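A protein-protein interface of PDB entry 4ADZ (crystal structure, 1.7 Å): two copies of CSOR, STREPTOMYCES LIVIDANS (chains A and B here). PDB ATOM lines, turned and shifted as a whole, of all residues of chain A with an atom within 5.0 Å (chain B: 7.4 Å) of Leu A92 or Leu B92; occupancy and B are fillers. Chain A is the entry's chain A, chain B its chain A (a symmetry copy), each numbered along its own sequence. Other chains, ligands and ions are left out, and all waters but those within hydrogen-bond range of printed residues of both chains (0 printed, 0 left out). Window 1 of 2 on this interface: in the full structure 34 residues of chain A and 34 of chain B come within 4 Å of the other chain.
Among the printed residues, pairs that only touch across the chains: Leu A58 with Ile B65 (3.9 Å), Leu A58 with Leu B68 (3.7 Å), Ile A61 with Ile B65 (3.96 Å), Ile A65 with Leu B58 (3.9 Å), Ile A65 with Ile B61 (3.96 Å), Ile A65 with Leu B92 (3.9 Å), Leu A68 with Leu B58 (3.7 Å), Leu A68 with Leu B92 (3.9 Å), Val A85 with Leu B92 (3.5 Å), Val A85 with Phe B95 (3.6 Å), Val A85 with Ala B96 (3.9 Å), Thr A89 with Leu B92 (3.5 Å), Lys A90 with Thr B136 (3.4 Å), Leu A92 with Ile B65 (3.9 Å), Leu A92 with Leu B68 (3.9 Å), Leu A92 with Val B85 (3.5 Å), Leu A92 with Thr B89 (3.5 Å), Leu A92 with Leu B92 (3.6 Å), Phe A95 with Val B85 (3.6 Å), Ala A96 with Leu B82 (3.5 Å) and Ala A96 with Val B85 (3.9 Å).
Printed residues of chain B within 4 Å of Leu A92: Ile B65, Leu B68, Val B85, Thr B89 and Leu B92. Of the printed residues of chain A, Leu B92 touches Ile A65, Leu A68, Val A85, Thr A89 and Leu A92. Of the printed residues of chain B, Thr A89 touches Leu B92 (3.5 Å) and Thr B136 (2.9 Å). Of the printed residues of chain B, Gln A93 touches Thr B136 (2.8 Å). Of the printed residues of chain A, Val B85 touches Leu A92, Phe A95 and Ala A96. Printed residues of chain B within 4 Å of Phe A95: Val B85 (3.6 Å). Of the printed residues of chain B, Val A85 touches Leu B92, Phe B95 and Ala B96. Lys B90 touches none of the printed residues of chain A. Ser B94 touches none of the printed residues of chain A. The nearest printed residue of chain B that does not touch Val A85 is Gln B93 (4.9 Å).
The side-chain hydroxyl (OG1) of Thr B136 lies close to the side-chain hydroxyl (OG1) of Thr A89 (3.1 Å). NE2 of Gln A93 sits at hydrogen-bond distance from O of Thr B136, 3.2 Å away.
Of the 14 printed residues of chain A, 11 touch a printed residue of chain B. Printed residues of chain A that touch a printed residue of chain B: Leu A58, Ile A61, Ile A65, Leu A68, Val A85, Thr A89, Lys A90, Leu A92, Gln A93, Phe A95 and Ala A96. Hydrophobic or aromatic side chains of chain A within 4 Å of the printed part of chain B: Leu A58, Ile A61, Ile A65, Leu A68, Val A85, Leu A92, Phe A95 and Ala A96. Along chain B the printed residues that touch a printed residue of chain A span positions 58 to 136. Among the printed residues, no Asp or Glu carboxylate lies within 4 Å of a Lys or Arg side-chain nitrogen of the other chain.
The backbone carbonyl oxygen (O) of Val B85 lies close to the side-chain hydroxyl (OG1) of Thr B89 (3.3 Å). The backbone carbonyl oxygen of Ser B86 is in hydrogen-bond range of the side-chain hydroxyl of Thr B89. The chain-end carboxylate (O) of Thr B136 lies within hydrogen-bond range of the side-chain amide nitrogen (NE2) of Gln B93, 3.0 Å away. O of Leu B82 is in hydrogen-bond range of OG of Ser B86, 3.4 Å away. The backbone carbonyl oxygen of Val A85 lies close to the side-chain hydroxyl of Thr A89.
Ile A65 touches Leu B92, and with the chains exchanged Leu A92 touches Ile B65. Val A85 touches Leu B92, and with the chains exchanged Leu A92 touches Val B85. Val A85 touches Ala B96, and with the chains exchanged Ala A96 touches Val B85. Leu A92 touches its own counterpart, Leu B92. Positions printed for both chains: 58, 61, 65, 68, 85, 88, 89, 90, 91, 92, 93, 94, 95 and 96. Of the 23 pairs that touch across the chains among the printed residues, 19 have their exchanged pair printed and touching as well.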
ATOM      1  N   LEU A  58      10.236 -20.629  15.375  1.00  0.00           N
ATOM      2  CA  LEU A  58      11.528 -21.271  15.189  1.00  0.00           C
ATOM      3  C   LEU A  58      12.129 -21.007  13.781  1.00  0.00           C
ATOM      4  O   LEU A  58      13.335 -20.957  13.613  1.00  0.00           O
ATOM      5  CB  LEU A  58      11.402 -22.781  15.455  1.00  0.00           C
ATOM      6  CG  LEU A  58      11.193 -23.119  16.928  1.00  0.00           C
ATOM      7  CD1 LEU A  58      10.801 -24.596  17.066  1.00  0.00           C
ATOM      8  CD2 LEU A  58      12.401 -22.784  17.830  1.00  0.00           C
ATOM      9  N   ILE A  61      13.794 -17.733  14.153  1.00  0.00           N
ATOM     10  CA  ILE A  61      15.061 -17.926  14.824  1.00  0.00           C
ATOM     11  C   ILE A  61      16.150 -18.559  13.963  1.00  0.00           C
ATOM     12  O   ILE A  61      17.271 -18.097  13.976  1.00  0.00           O
ATOM     13  CB  ILE A  61      14.897 -18.739  16.156  1.00  0.00           C
ATOM     14  CG1 ILE A  61      14.010 -17.931  17.160  1.00  0.00           C
ATOM     15  CG2 ILE A  61      16.289 -19.210  16.680  1.00  0.00           C
ATOM     16  CD1 ILE A  61      13.290 -18.788  18.221  1.00  0.00           C
ATOM     17  N   ILE A  65      19.974 -17.145  12.953  1.00  0.00           N
ATOM     18  CA  ILE A  65      21.199 -17.831  13.071  1.00  0.00           C
ATOM     19  C   ILE A  65      21.908 -17.858  11.698  1.00  0.00           C
ATOM     20  O   ILE A  65      23.153 -17.742  11.619  1.00  0.00           O
ATOM     21  CB  ILE A  65      21.075 -19.259  13.617  1.00  0.00           C
ATOM     22  CG1 ILE A  65      20.251 -19.315  14.899  1.00  0.00           C
ATOM     23  CG2 ILE A  65      22.447 -19.882  13.805  1.00  0.00           C
ATOM     24  CD1 ILE A  65      20.747 -18.431  16.058  1.00  0.00           C
ATOM     25  N   LEU A  68      23.552 -14.620  11.496  1.00  0.00           N
ATOM     26  CA  LEU A  68      24.801 -14.633  12.221  1.00  0.00           C
ATOM     27  C   LEU A  68      25.945 -15.265  11.427  1.00  0.00           C
ATOM     28  O   LEU A  68      27.096 -14.788  11.457  1.00  0.00           O
ATOM     29  CB  LEU A  68      24.659 -15.388  13.552  1.00  0.00           C
ATOM     30  CG  LEU A  68      23.868 -14.647  14.617  1.00  0.00           C
ATOM     31  CD1 LEU A  68      23.560 -15.630  15.764  1.00  0.00           C
ATOM     32  CD2 LEU A  68      24.631 -13.387  15.042  1.00  0.00           C
ATOM     33  N   VAL A  85      23.120 -11.657  18.250  1.00  0.00           N
ATOM     34  CA  VAL A  85      23.128 -12.824  19.180  1.00  0.00           C
ATOM     35  C   VAL A  85      22.066 -12.573  20.266  1.00  0.00           C
ATOM     36  O   VAL A  85      21.252 -13.482  20.636  1.00  0.00           O
ATOM     37  CB  VAL A  85      24.478 -13.173  19.783  1.00  0.00           C
ATOM     38  CG1 VAL A  85      24.407 -14.263  20.941  1.00  0.00           C
ATOM     39  CG2 VAL A  85      25.503 -13.587  18.689  1.00  0.00           C
ATOM     40  N   SER A  88      18.594 -13.042  19.089  1.00  0.00           N
ATOM     41  CA  SER A  88      18.263 -14.476  18.896  1.00  0.00           C
ATOM     42  C   SER A  88      18.035 -15.173  20.231  1.00  0.00           C
ATOM     43  O   SER A  88      17.098 -15.942  20.382  1.00  0.00           O
ATOM     44  CB  SER A  88      19.371 -15.165  18.139  1.00  0.00           C
ATOM     45  OG  SER A  88      19.585 -14.481  16.908  1.00  0.00           O
ATOM     46  N   THR A  89      18.816 -14.840  21.233  1.00  0.00           N
ATOM     47  CA  THR A  89      18.632 -15.431  22.587  1.00  0.00           C
ATOM     48  C   THR A  89      17.302 -14.970  23.160  1.00  0.00           C
ATOM     49  O   THR A  89      16.533 -15.771  23.735  1.00  0.00           O
ATOM     50  CB  THR A  89      19.831 -15.158  23.546  1.00  0.00           C
ATOM     51  OG1 THR A  89      20.031 -13.745  23.731  1.00  0.00           O
ATOM     52  CG2 THR A  89      21.114 -15.766  23.008  1.00  0.00           C
ATOM     53  N   LYS A  90      16.993 -13.689  22.987  1.00  0.00           N
ATOM     54  CA  LYS A  90      15.709 -13.156  23.431  1.00  0.00           C
ATOM     55  C   LYS A  90      14.556 -13.873  22.785  1.00  0.00           C
ATOM     56  O   LYS A  90      13.587 -14.212  23.490  1.00  0.00           O
ATOM     57  CB  LYS A  90      15.662 -11.624  23.233  1.00  0.00           C
ATOM     58  CG  LYS A  90      14.342 -10.941  23.538  1.00  0.00           C
ATOM     59  CD  LYS A  90      14.250  -9.510  22.967  1.00  0.00           C
ATOM     60  CE  LYS A  90      12.988  -8.788  23.424  1.00  0.00           C
ATOM     61  NZ  LYS A  90      12.955  -8.671  24.905  1.00  0.00           N
ATOM     62  N   ALA A  91      14.632 -14.146  21.477  1.00  0.00           N
ATOM     63  CA  ALA A  91      13.566 -14.853  20.764  1.00  0.00           C
ATOM     64  C   ALA A  91      13.384 -16.285  21.279  1.00  0.00           C
ATOM     65  O   ALA A  91      12.268 -16.768  21.442  1.00  0.00           O
ATOM     66  CB  ALA A  91      13.843 -14.904  19.263  1.00  0.00           C
ATOM     67  N   LEU A  92      14.496 -16.915  21.555  1.00  0.00           N
ATOM     68  CA  LEU A  92      14.450 -18.300  22.144  1.00  0.00           C
ATOM     69  C   LEU A  92      13.792 -18.283  23.515  1.00  0.00           C
ATOM     70  O   LEU A  92      13.042 -19.222  23.842  1.00  0.00           O
ATOM     71  CB  LEU A  92      15.842 -18.928  22.220  1.00  0.00           C
ATOM     72  CG  LEU A  92      16.342 -19.540  20.915  1.00  0.00           C
ATOM     73  CD1 LEU A  92      17.848 -19.619  20.894  1.00  0.00           C
ATOM     74  CD2 LEU A  92      15.693 -20.913  20.555  1.00  0.00           C
ATOM     75  N   GLN A  93      14.107 -17.284  24.310  1.00  0.00           N
ATOM     76  CA  GLN A  93      13.518 -17.147  25.663  1.00  0.00           C
ATOM     77  C   GLN A  93      12.024 -16.911  25.571  1.00  0.00           C
ATOM     78  O   GLN A  93      11.230 -17.535  26.321  1.00  0.00           O
ATOM     79  CB  GLN A  93      14.197 -16.056  26.458  1.00  0.00           C
ATOM     80  CG  GLN A  93      15.615 -16.395  26.890  1.00  0.00           C
ATOM     81  CD  GLN A  93      16.266 -15.224  27.662  1.00  0.00           C
ATOM     82  OE1 GLN A  93      15.981 -14.045  27.416  1.00  0.00           O
ATOM     83  NE2 GLN A  93      17.017 -15.561  28.687  1.00  0.00           N
ATOM     84  N   SER A  94      11.601 -16.095  24.596  1.00  0.00           N
ATOM     85  CA  SER A  94      10.211 -15.783  24.427  1.00  0.00           C
ATOM     86  C   SER A  94       9.478 -17.049  24.005  1.00  0.00           C
ATOM     87  O   SER A  94       8.375 -17.269  24.466  1.00  0.00           O
ATOM     88  CB  SER A  94       9.973 -14.692  23.371  1.00  0.00           C
ATOM     89  OG  SER A  94       8.582 -14.551  23.059  1.00  0.00           O
ATOM     90  N   PHE A  95      10.077 -17.815  23.093  1.00  0.00           N
ATOM     91  CA  PHE A  95       9.557 -19.149  22.644  1.00  0.00           C
ATOM     92  C   PHE A  95       9.403 -20.090  23.874  1.00  0.00           C
ATOM     93  O   PHE A  95       8.330 -20.716  24.084  1.00  0.00           O
ATOM     94  CB  PHE A  95      10.503 -19.762  21.595  1.00  0.00           C
ATOM     95  CG  PHE A  95      10.190 -21.206  21.227  1.00  0.00           C
ATOM     96  CD1 PHE A  95       9.158 -21.527  20.358  1.00  0.00           C
ATOM     97  CD2 PHE A  95      10.946 -22.229  21.728  1.00  0.00           C
ATOM     98  CE1 PHE A  95       8.881 -22.863  20.038  1.00  0.00           C
ATOM     99  CE2 PHE A  95      10.697 -23.565  21.388  1.00  0.00           C
ATOM    100  CZ  PHE A  95       9.659 -23.874  20.557  1.00  0.00           C
ATOM    101  N   ALA A  96      10.409 -20.129  24.720  1.00  0.00           N
ATOM    102  CA  ALA A  96      10.422 -21.015  25.909  1.00  0.00           C
ATOM    103  C   ALA A  96       9.257 -20.621  26.847  1.00  0.00           C
ATOM    104  O   ALA A  96       8.508 -21.480  27.332  1.00  0.00           O
ATOM    105  CB  ALA A  96      11.757 -20.929  26.640  1.00  0.00           C
ATOM    106  N   ARG B  57      30.886 -23.168  15.463  1.00  0.00           N
ATOM    107  CA  ARG B  57      29.934 -22.970  16.595  1.00  0.00           C
ATOM    108  C   ARG B  57      28.521 -22.642  16.073  1.00  0.00           C
ATOM    109  O   ARG B  57      27.538 -23.177  16.570  1.00  0.00           O
ATOM    110  CB  ARG B  57      30.446 -21.845  17.520  1.00  0.00           C
ATOM    111  CG  ARG B  57      31.608 -22.230  18.418  1.00  0.00           C
ATOM    112  CD  ARG B  57      32.082 -21.009  19.179  1.00  0.00           C
ATOM    113  NE  ARG B  57      32.992 -21.252  20.283  1.00  0.00           N
ATOM    114  CZ  ARG B  57      32.646 -21.373  21.562  1.00  0.00           C
ATOM    115  NH1 ARG B  57      31.382 -21.350  21.987  1.00  0.00           N
ATOM    116  NH2 ARG B  57      33.620 -21.554  22.432  1.00  0.00           N
ATOM    117  N   LEU B  58      28.390 -21.777  15.069  1.00  0.00           N
ATOM    118  CA  LEU B  58      27.070 -21.405  14.584  1.00  0.00           C
ATOM    119  C   LEU B  58      26.375 -22.554  13.802  1.00  0.00           C
ATOM    120  O   LEU B  58      25.163 -22.671  13.805  1.00  0.00           O
ATOM    121  CB  LEU B  58      27.170 -20.137  13.720  1.00  0.00           C
ATOM    122  CG  LEU B  58      27.476 -18.879  14.526  1.00  0.00           C
ATOM    123  CD1 LEU B  58      27.833 -17.732  13.573  1.00  0.00           C
ATOM    124  CD2 LEU B  58      26.346 -18.459  15.494  1.00  0.00           C
ATOM    125  N   ILE B  61      24.839 -24.605  16.460  1.00  0.00           N
ATOM    126  CA  ILE B  61      23.619 -23.963  16.899  1.00  0.00           C
ATOM    127  C   ILE B  61      22.452 -24.073  15.922  1.00  0.00           C
ATOM    128  O   ILE B  61      21.349 -24.364  16.333  1.00  0.00           O
ATOM    129  CB  ILE B  61      23.855 -22.459  17.279  1.00  0.00           C
ATOM    130  CG1 ILE B  61      24.836 -22.372  18.495  1.00  0.00           C
ATOM    131  CG2 ILE B  61      22.492 -21.716  17.429  1.00  0.00           C
ATOM    132  CD1 ILE B  61      25.607 -21.040  18.609  1.00  0.00           C
ATOM    133  N   GLN B  64      20.927 -27.330  16.342  1.00  0.00           N
ATOM    134  CA  GLN B  64      20.036 -27.341  17.529  1.00  0.00           C
ATOM    135  C   GLN B  64      18.680 -26.772  17.227  1.00  0.00           C
ATOM    136  O   GLN B  64      17.680 -27.295  17.663  1.00  0.00           O
ATOM    137  CB  GLN B  64      20.727 -26.630  18.704  1.00  0.00           C
ATOM    138  CG  GLN B  64      21.983 -27.322  19.247  1.00  0.00           C
ATOM    139  CD  GLN B  64      22.615 -26.432  20.313  1.00  0.00           C
ATOM    140  OE1 GLN B  64      22.921 -25.294  20.046  1.00  0.00           O
ATOM    141  NE2 GLN B  64      22.716 -26.921  21.547  1.00  0.00           N
ATOM    142  N   ILE B  65      18.608 -25.679  16.456  1.00  0.00           N
ATOM    143  CA  ILE B  65      17.375 -25.067  16.154  1.00  0.00           C
ATOM    144  C   ILE B  65      16.567 -25.978  15.203  1.00  0.00           C
ATOM    145  O   ILE B  65      15.324 -26.080  15.317  1.00  0.00           O
ATOM    146  CB  ILE B  65      17.497 -23.664  15.547  1.00  0.00           C
ATOM    147  CG1 ILE B  65      18.409 -22.759  16.368  1.00  0.00           C
ATOM    148  CG2 ILE B  65      16.124 -23.044  15.349  1.00  0.00           C
ATOM    149  CD1 ILE B  65      18.025 -22.577  17.847  1.00  0.00           C
ATOM    150  N   LEU B  68      15.009 -28.402  17.421  1.00  0.00           N
ATOM    151  CA  LEU B  68      13.817 -27.854  18.023  1.00  0.00           C
ATOM    152  C   LEU B  68      12.599 -27.915  17.099  1.00  0.00           C
ATOM    153  O   LEU B  68      11.468 -28.204  17.536  1.00  0.00           O
ATOM    154  CB  LEU B  68      14.032 -26.391  18.445  1.00  0.00           C
ATOM    155  CG  LEU B  68      14.921 -26.210  19.665  1.00  0.00           C
ATOM    156  CD1 LEU B  68      15.282 -24.716  19.783  1.00  0.00           C
ATOM    157  CD2 LEU B  68      14.228 -26.800  20.898  1.00  0.00           C
ATOM    158  N   LEU B  82      12.078 -27.496  26.168  1.00  0.00           N
ATOM    159  CA  LEU B  82      12.712 -26.468  27.006  1.00  0.00           C
ATOM    160  C   LEU B  82      14.136 -26.776  27.334  1.00  0.00           C
ATOM    161  O   LEU B  82      15.017 -25.908  27.228  1.00  0.00           O
ATOM    162  CB  LEU B  82      11.913 -26.194  28.267  1.00  0.00           C
ATOM    163  CG  LEU B  82      10.520 -25.631  28.100  1.00  0.00           C
ATOM    164  CD1 LEU B  82       9.806 -25.435  29.470  1.00  0.00           C
ATOM    165  CD2 LEU B  82      10.548 -24.327  27.345  1.00  0.00           C
ATOM    166  N   GLN B  84      16.290 -28.391  25.472  1.00  0.00           N
ATOM    167  CA  GLN B  84      17.035 -28.127  24.244  1.00  0.00           C
ATOM    168  C   GLN B  84      17.082 -26.599  23.963  1.00  0.00           C
ATOM    169  O   GLN B  84      18.105 -26.129  23.459  1.00  0.00           O
ATOM    170  CB  GLN B  84      16.350 -28.827  23.087  1.00  0.00           C
ATOM    171  CG  GLN B  84      16.924 -28.553  21.721  1.00  0.00           C
ATOM    172  CD  GLN B  84      18.182 -29.293  21.383  1.00  0.00           C
ATOM    173  OE1 GLN B  84      18.829 -29.990  22.242  1.00  0.00           O
ATOM    174  NE2 GLN B  84      18.539 -29.200  20.053  1.00  0.00           N
ATOM    175  N   VAL B  85      16.018 -25.867  24.288  1.00  0.00           N
ATOM    176  CA  VAL B  85      16.043 -24.382  24.146  1.00  0.00           C
ATOM    177  C   VAL B  85      17.188 -23.840  25.021  1.00  0.00           C
ATOM    178  O   VAL B  85      18.001 -22.953  24.598  1.00  0.00           O
ATOM    179  CB  VAL B  85      14.731 -23.672  24.435  1.00  0.00           C
ATOM    180  CG1 VAL B  85      14.854 -22.087  24.504  1.00  0.00           C
ATOM    181  CG2 VAL B  85      13.618 -24.102  23.437  1.00  0.00           C
ATOM    182  N   SER B  86      17.294 -24.325  26.260  1.00  0.00           N
ATOM    183  CA  SER B  86      18.265 -23.811  27.201  1.00  0.00           C
ATOM    184  C   SER B  86      19.661 -24.169  26.718  1.00  0.00           C
ATOM    185  O   SER B  86      20.587 -23.337  26.771  1.00  0.00           O
ATOM    186  CB  SER B  86      17.963 -24.381  28.628  1.00  0.00           C
ATOM    187  OG  SER B  86      16.778 -23.778  29.130  1.00  0.00           O
ATOM    188  N   ALA B  87      19.841 -25.360  26.162  1.00  0.00           N
ATOM    189  CA  ALA B  87      21.104 -25.705  25.596  1.00  0.00           C
ATOM    190  C   ALA B  87      21.499 -24.761  24.442  1.00  0.00           C
ATOM    191  O   ALA B  87      22.691 -24.425  24.333  1.00  0.00           O
ATOM    192  CB  ALA B  87      21.168 -27.157  25.142  1.00  0.00           C
ATOM    193  N   SER B  88      20.551 -24.420  23.599  1.00  0.00           N
ATOM    194  CA  SER B  88      20.824 -23.531  22.443  1.00  0.00           C
ATOM    195  C   SER B  88      21.128 -22.111  22.901  1.00  0.00           C
ATOM    196  O   SER B  88      22.051 -21.479  22.408  1.00  0.00           O
ATOM    197  CB  SER B  88      19.645 -23.527  21.504  1.00  0.00           C
ATOM    198  OG  SER B  88      19.362 -24.868  21.110  1.00  0.00           O
ATOM    199  N   THR B  89      20.432 -21.633  23.907  1.00  0.00           N
ATOM    200  CA  THR B  89      20.697 -20.274  24.454  1.00  0.00           C
ATOM    201  C   THR B  89      22.078 -20.248  25.089  1.00  0.00           C
ATOM    202  O   THR B  89      22.863 -19.295  24.890  1.00  0.00           O
ATOM    203  CB  THR B  89      19.579 -19.771  25.419  1.00  0.00           C
ATOM    204  OG1 THR B  89      19.435 -20.654  26.545  1.00  0.00           O
ATOM    205  CG2 THR B  89      18.243 -19.668  24.705  1.00  0.00           C
ATOM    206  N   LYS B  90      22.411 -21.300  25.831  1.00  0.00           N
ATOM    207  CA  LYS B  90      23.739 -21.413  26.424  1.00  0.00           C
ATOM    208  C   LYS B  90      24.821 -21.378  25.380  1.00  0.00           C
ATOM    209  O   LYS B  90      25.827 -20.674  25.580  1.00  0.00           O
ATOM    210  CB  LYS B  90      23.817 -22.655  27.341  1.00  0.00           C
ATOM    211  CG  LYS B  90      25.174 -22.974  27.937  1.00  0.00           C
ATOM    212  CD  LYS B  90      25.267 -24.404  28.514  1.00  0.00           C
ATOM    213  CE  LYS B  90      26.579 -24.644  29.250  1.00  0.00           C
ATOM    214  NZ  LYS B  90      26.723 -23.703  30.390  1.00  0.00           N
ATOM    215  N   ALA B  91      24.642 -22.086  24.259  1.00  0.00           N
ATOM    216  CA  ALA B  91      25.631 -22.102  23.180  1.00  0.00           C
ATOM    217  C   ALA B  91      25.808 -20.720  22.543  1.00  0.00           C
ATOM    218  O   ALA B  91      26.919 -20.292  22.245  1.00  0.00           O
ATOM    219  CB  ALA B  91      25.245 -23.098  22.088  1.00  0.00           C
ATOM    220  N   LEU B  92      24.702 -20.042  22.385  1.00  0.00           N
ATOM    221  CA  LEU B  92      24.749 -18.638  21.844  1.00  0.00           C
ATOM    222  C   LEU B  92      25.506 -17.719  22.792  1.00  0.00           C
ATOM    223  O   LEU B  92      26.250 -16.838  22.320  1.00  0.00           O
ATOM    224  CB  LEU B  92      23.349 -18.092  21.565  1.00  0.00           C
ATOM    225  CG  LEU B  92      22.738 -18.542  20.241  1.00  0.00           C
ATOM    226  CD1 LEU B  92      21.232 -18.455  20.280  1.00  0.00           C
ATOM    227  CD2 LEU B  92      23.318 -17.821  18.984  1.00  0.00           C
ATOM    228  N   GLN B  93      25.279 -17.879  24.077  1.00  0.00           N
ATOM    229  CA  GLN B  93      25.969 -17.056  25.099  1.00  0.00           C
ATOM    230  C   GLN B  93      27.458 -17.334  25.089  1.00  0.00           C
ATOM    231  O   GLN B  93      28.286 -16.388  25.136  1.00  0.00           O
ATOM    232  CB  GLN B  93      25.382 -17.271  26.475  1.00  0.00           C
ATOM    233  CG  GLN B  93      23.989 -16.686  26.652  1.00  0.00           C
ATOM    234  CD  GLN B  93      23.431 -16.975  28.065  1.00  0.00           C
ATOM    235  OE1 GLN B  93      23.731 -18.002  28.685  1.00  0.00           O
ATOM    236  NE2 GLN B  93      22.747 -15.999  28.622  1.00  0.00           N
ATOM    237  N   SER B  94      27.832 -18.609  24.924  1.00  0.00           N
ATOM    238  CA  SER B  94      29.215 -18.992  24.917  1.00  0.00           C
ATOM    239  C   SER B  94      29.878 -18.395  23.684  1.00  0.00           C
ATOM    240  O   SER B  94      31.005 -17.949  23.783  1.00  0.00           O
ATOM    241  CB  SER B  94      29.408 -20.517  24.900  1.00  0.00           C
ATOM    242  OG  SER B  94      30.776 -20.875  24.673  1.00  0.00           O
ATOM    243  N   PHE B  95      29.193 -18.458  22.543  1.00  0.00           N
ATOM    244  CA  PHE B  95      29.639 -17.824  21.258  1.00  0.00           C
ATOM    245  C   PHE B  95      29.854 -16.298  21.477  1.00  0.00           C
ATOM    246  O   PHE B  95      30.921 -15.733  21.115  1.00  0.00           O
ATOM    247  CB  PHE B  95      28.601 -18.082  20.150  1.00  0.00           C
ATOM    248  CG  PHE B  95      28.844 -17.306  18.862  1.00  0.00           C
ATOM    249  CD1 PHE B  95      29.801 -17.707  17.941  1.00  0.00           C
ATOM    250  CD2 PHE B  95      28.097 -16.200  18.568  1.00  0.00           C
ATOM    251  CE1 PHE B  95      30.014 -16.975  16.766  1.00  0.00           C
ATOM    252  CE2 PHE B  95      28.282 -15.481  17.380  1.00  0.00           C
ATOM    253  CZ  PHE B  95      29.247 -15.865  16.494  1.00  0.00           C
ATOM    254  N   ALA B  96      28.911 -15.653  22.130  1.00  0.00           N
ATOM    255  CA  ALA B  96      28.959 -14.191  22.369  1.00  0.00           C
ATOM    256  C   ALA B  96      30.200 -13.859  23.230  1.00  0.00           C
ATOM    257  O   ALA B  96      30.957 -12.926  22.928  1.00  0.00           O
ATOM    258  CB  ALA B  96      27.684 -13.707  23.049  1.00  0.00           C
ATOM    259  N   LEU B  97      30.458 -14.669  24.240  1.00  0.00           N
ATOM    260  CA  LEU B  97      31.599 -14.422  25.135  1.00  0.00           C
ATOM    261  C   LEU B  97      32.913 -14.577  24.436  1.00  0.00           C
ATOM    262  O   LEU B  97      33.860 -13.823  24.689  1.00  0.00           O
ATOM    263  CB  LEU B  97      31.547 -15.322  26.358  1.00  0.00           C
ATOM    264  CG  LEU B  97      30.492 -15.037  27.392  1.00  0.00           C
ATOM    265  CD1 LEU B  97      30.282 -16.257  28.319  1.00  0.00           C
ATOM    266  CD2 LEU B  97      30.903 -13.811  28.189  1.00  0.00           C
ATOM    267  N   GLN B  98      33.000 -15.541  23.533  1.00  0.00           N
ATOM    268  CA  GLN B  98      34.203 -15.738  22.743  1.00  0.00           C
ATOM    269  C   GLN B  98      34.463 -14.529  21.836  1.00  0.00           C
ATOM    270  O   GLN B  98      35.608 -14.046  21.726  1.00  0.00           O
ATOM    271  CB  GLN B  98      34.083 -16.983  21.894  1.00  0.00           C
ATOM    272  CG  GLN B  98      34.345 -18.255  22.696  1.00  0.00           C
ATOM    273  N   LEU B 133      23.633  -8.430  26.638  1.00  0.00           N
ATOM    274  CA  LEU B 133      23.881  -9.859  26.885  1.00  0.00           C
ATOM    275  C   LEU B 133      23.361 -10.318  28.248  1.00  0.00           C
ATOM    276  O   LEU B 133      22.716 -11.398  28.364  1.00  0.00           O
ATOM    277  CB  LEU B 133      25.364 -10.181  26.778  1.00  0.00           C
ATOM    278  CG  LEU B 133      25.897 -11.614  26.880  1.00  0.00           C
ATOM    279  CD1 LEU B 133      25.139 -12.565  25.964  1.00  0.00           C
ATOM    280  CD2 LEU B 133      27.382 -11.640  26.493  1.00  0.00           C
ATOM    281  N   THR B 136      19.565 -11.130  28.596  1.00  0.00           N
ATOM    282  CA  THR B 136      19.098 -12.449  28.178  1.00  0.00           C
ATOM    283  C   THR B 136      19.678 -13.455  29.191  1.00  0.00           C
ATOM    284  O   THR B 136      20.079 -14.565  28.852  1.00  0.00           O
ATOM    285  CB  THR B 136      19.487 -12.798  26.713  1.00  0.00           C
ATOM    286  OG1 THR B 136      19.642 -11.605  25.900  1.00  0.00           O
ATOM    287  CG2 THR B 136      18.448 -13.681  26.111  1.00  0.00           C
ATOM    288  OXT THR B 136      19.762 -13.195  30.417  1.00  0.00           O
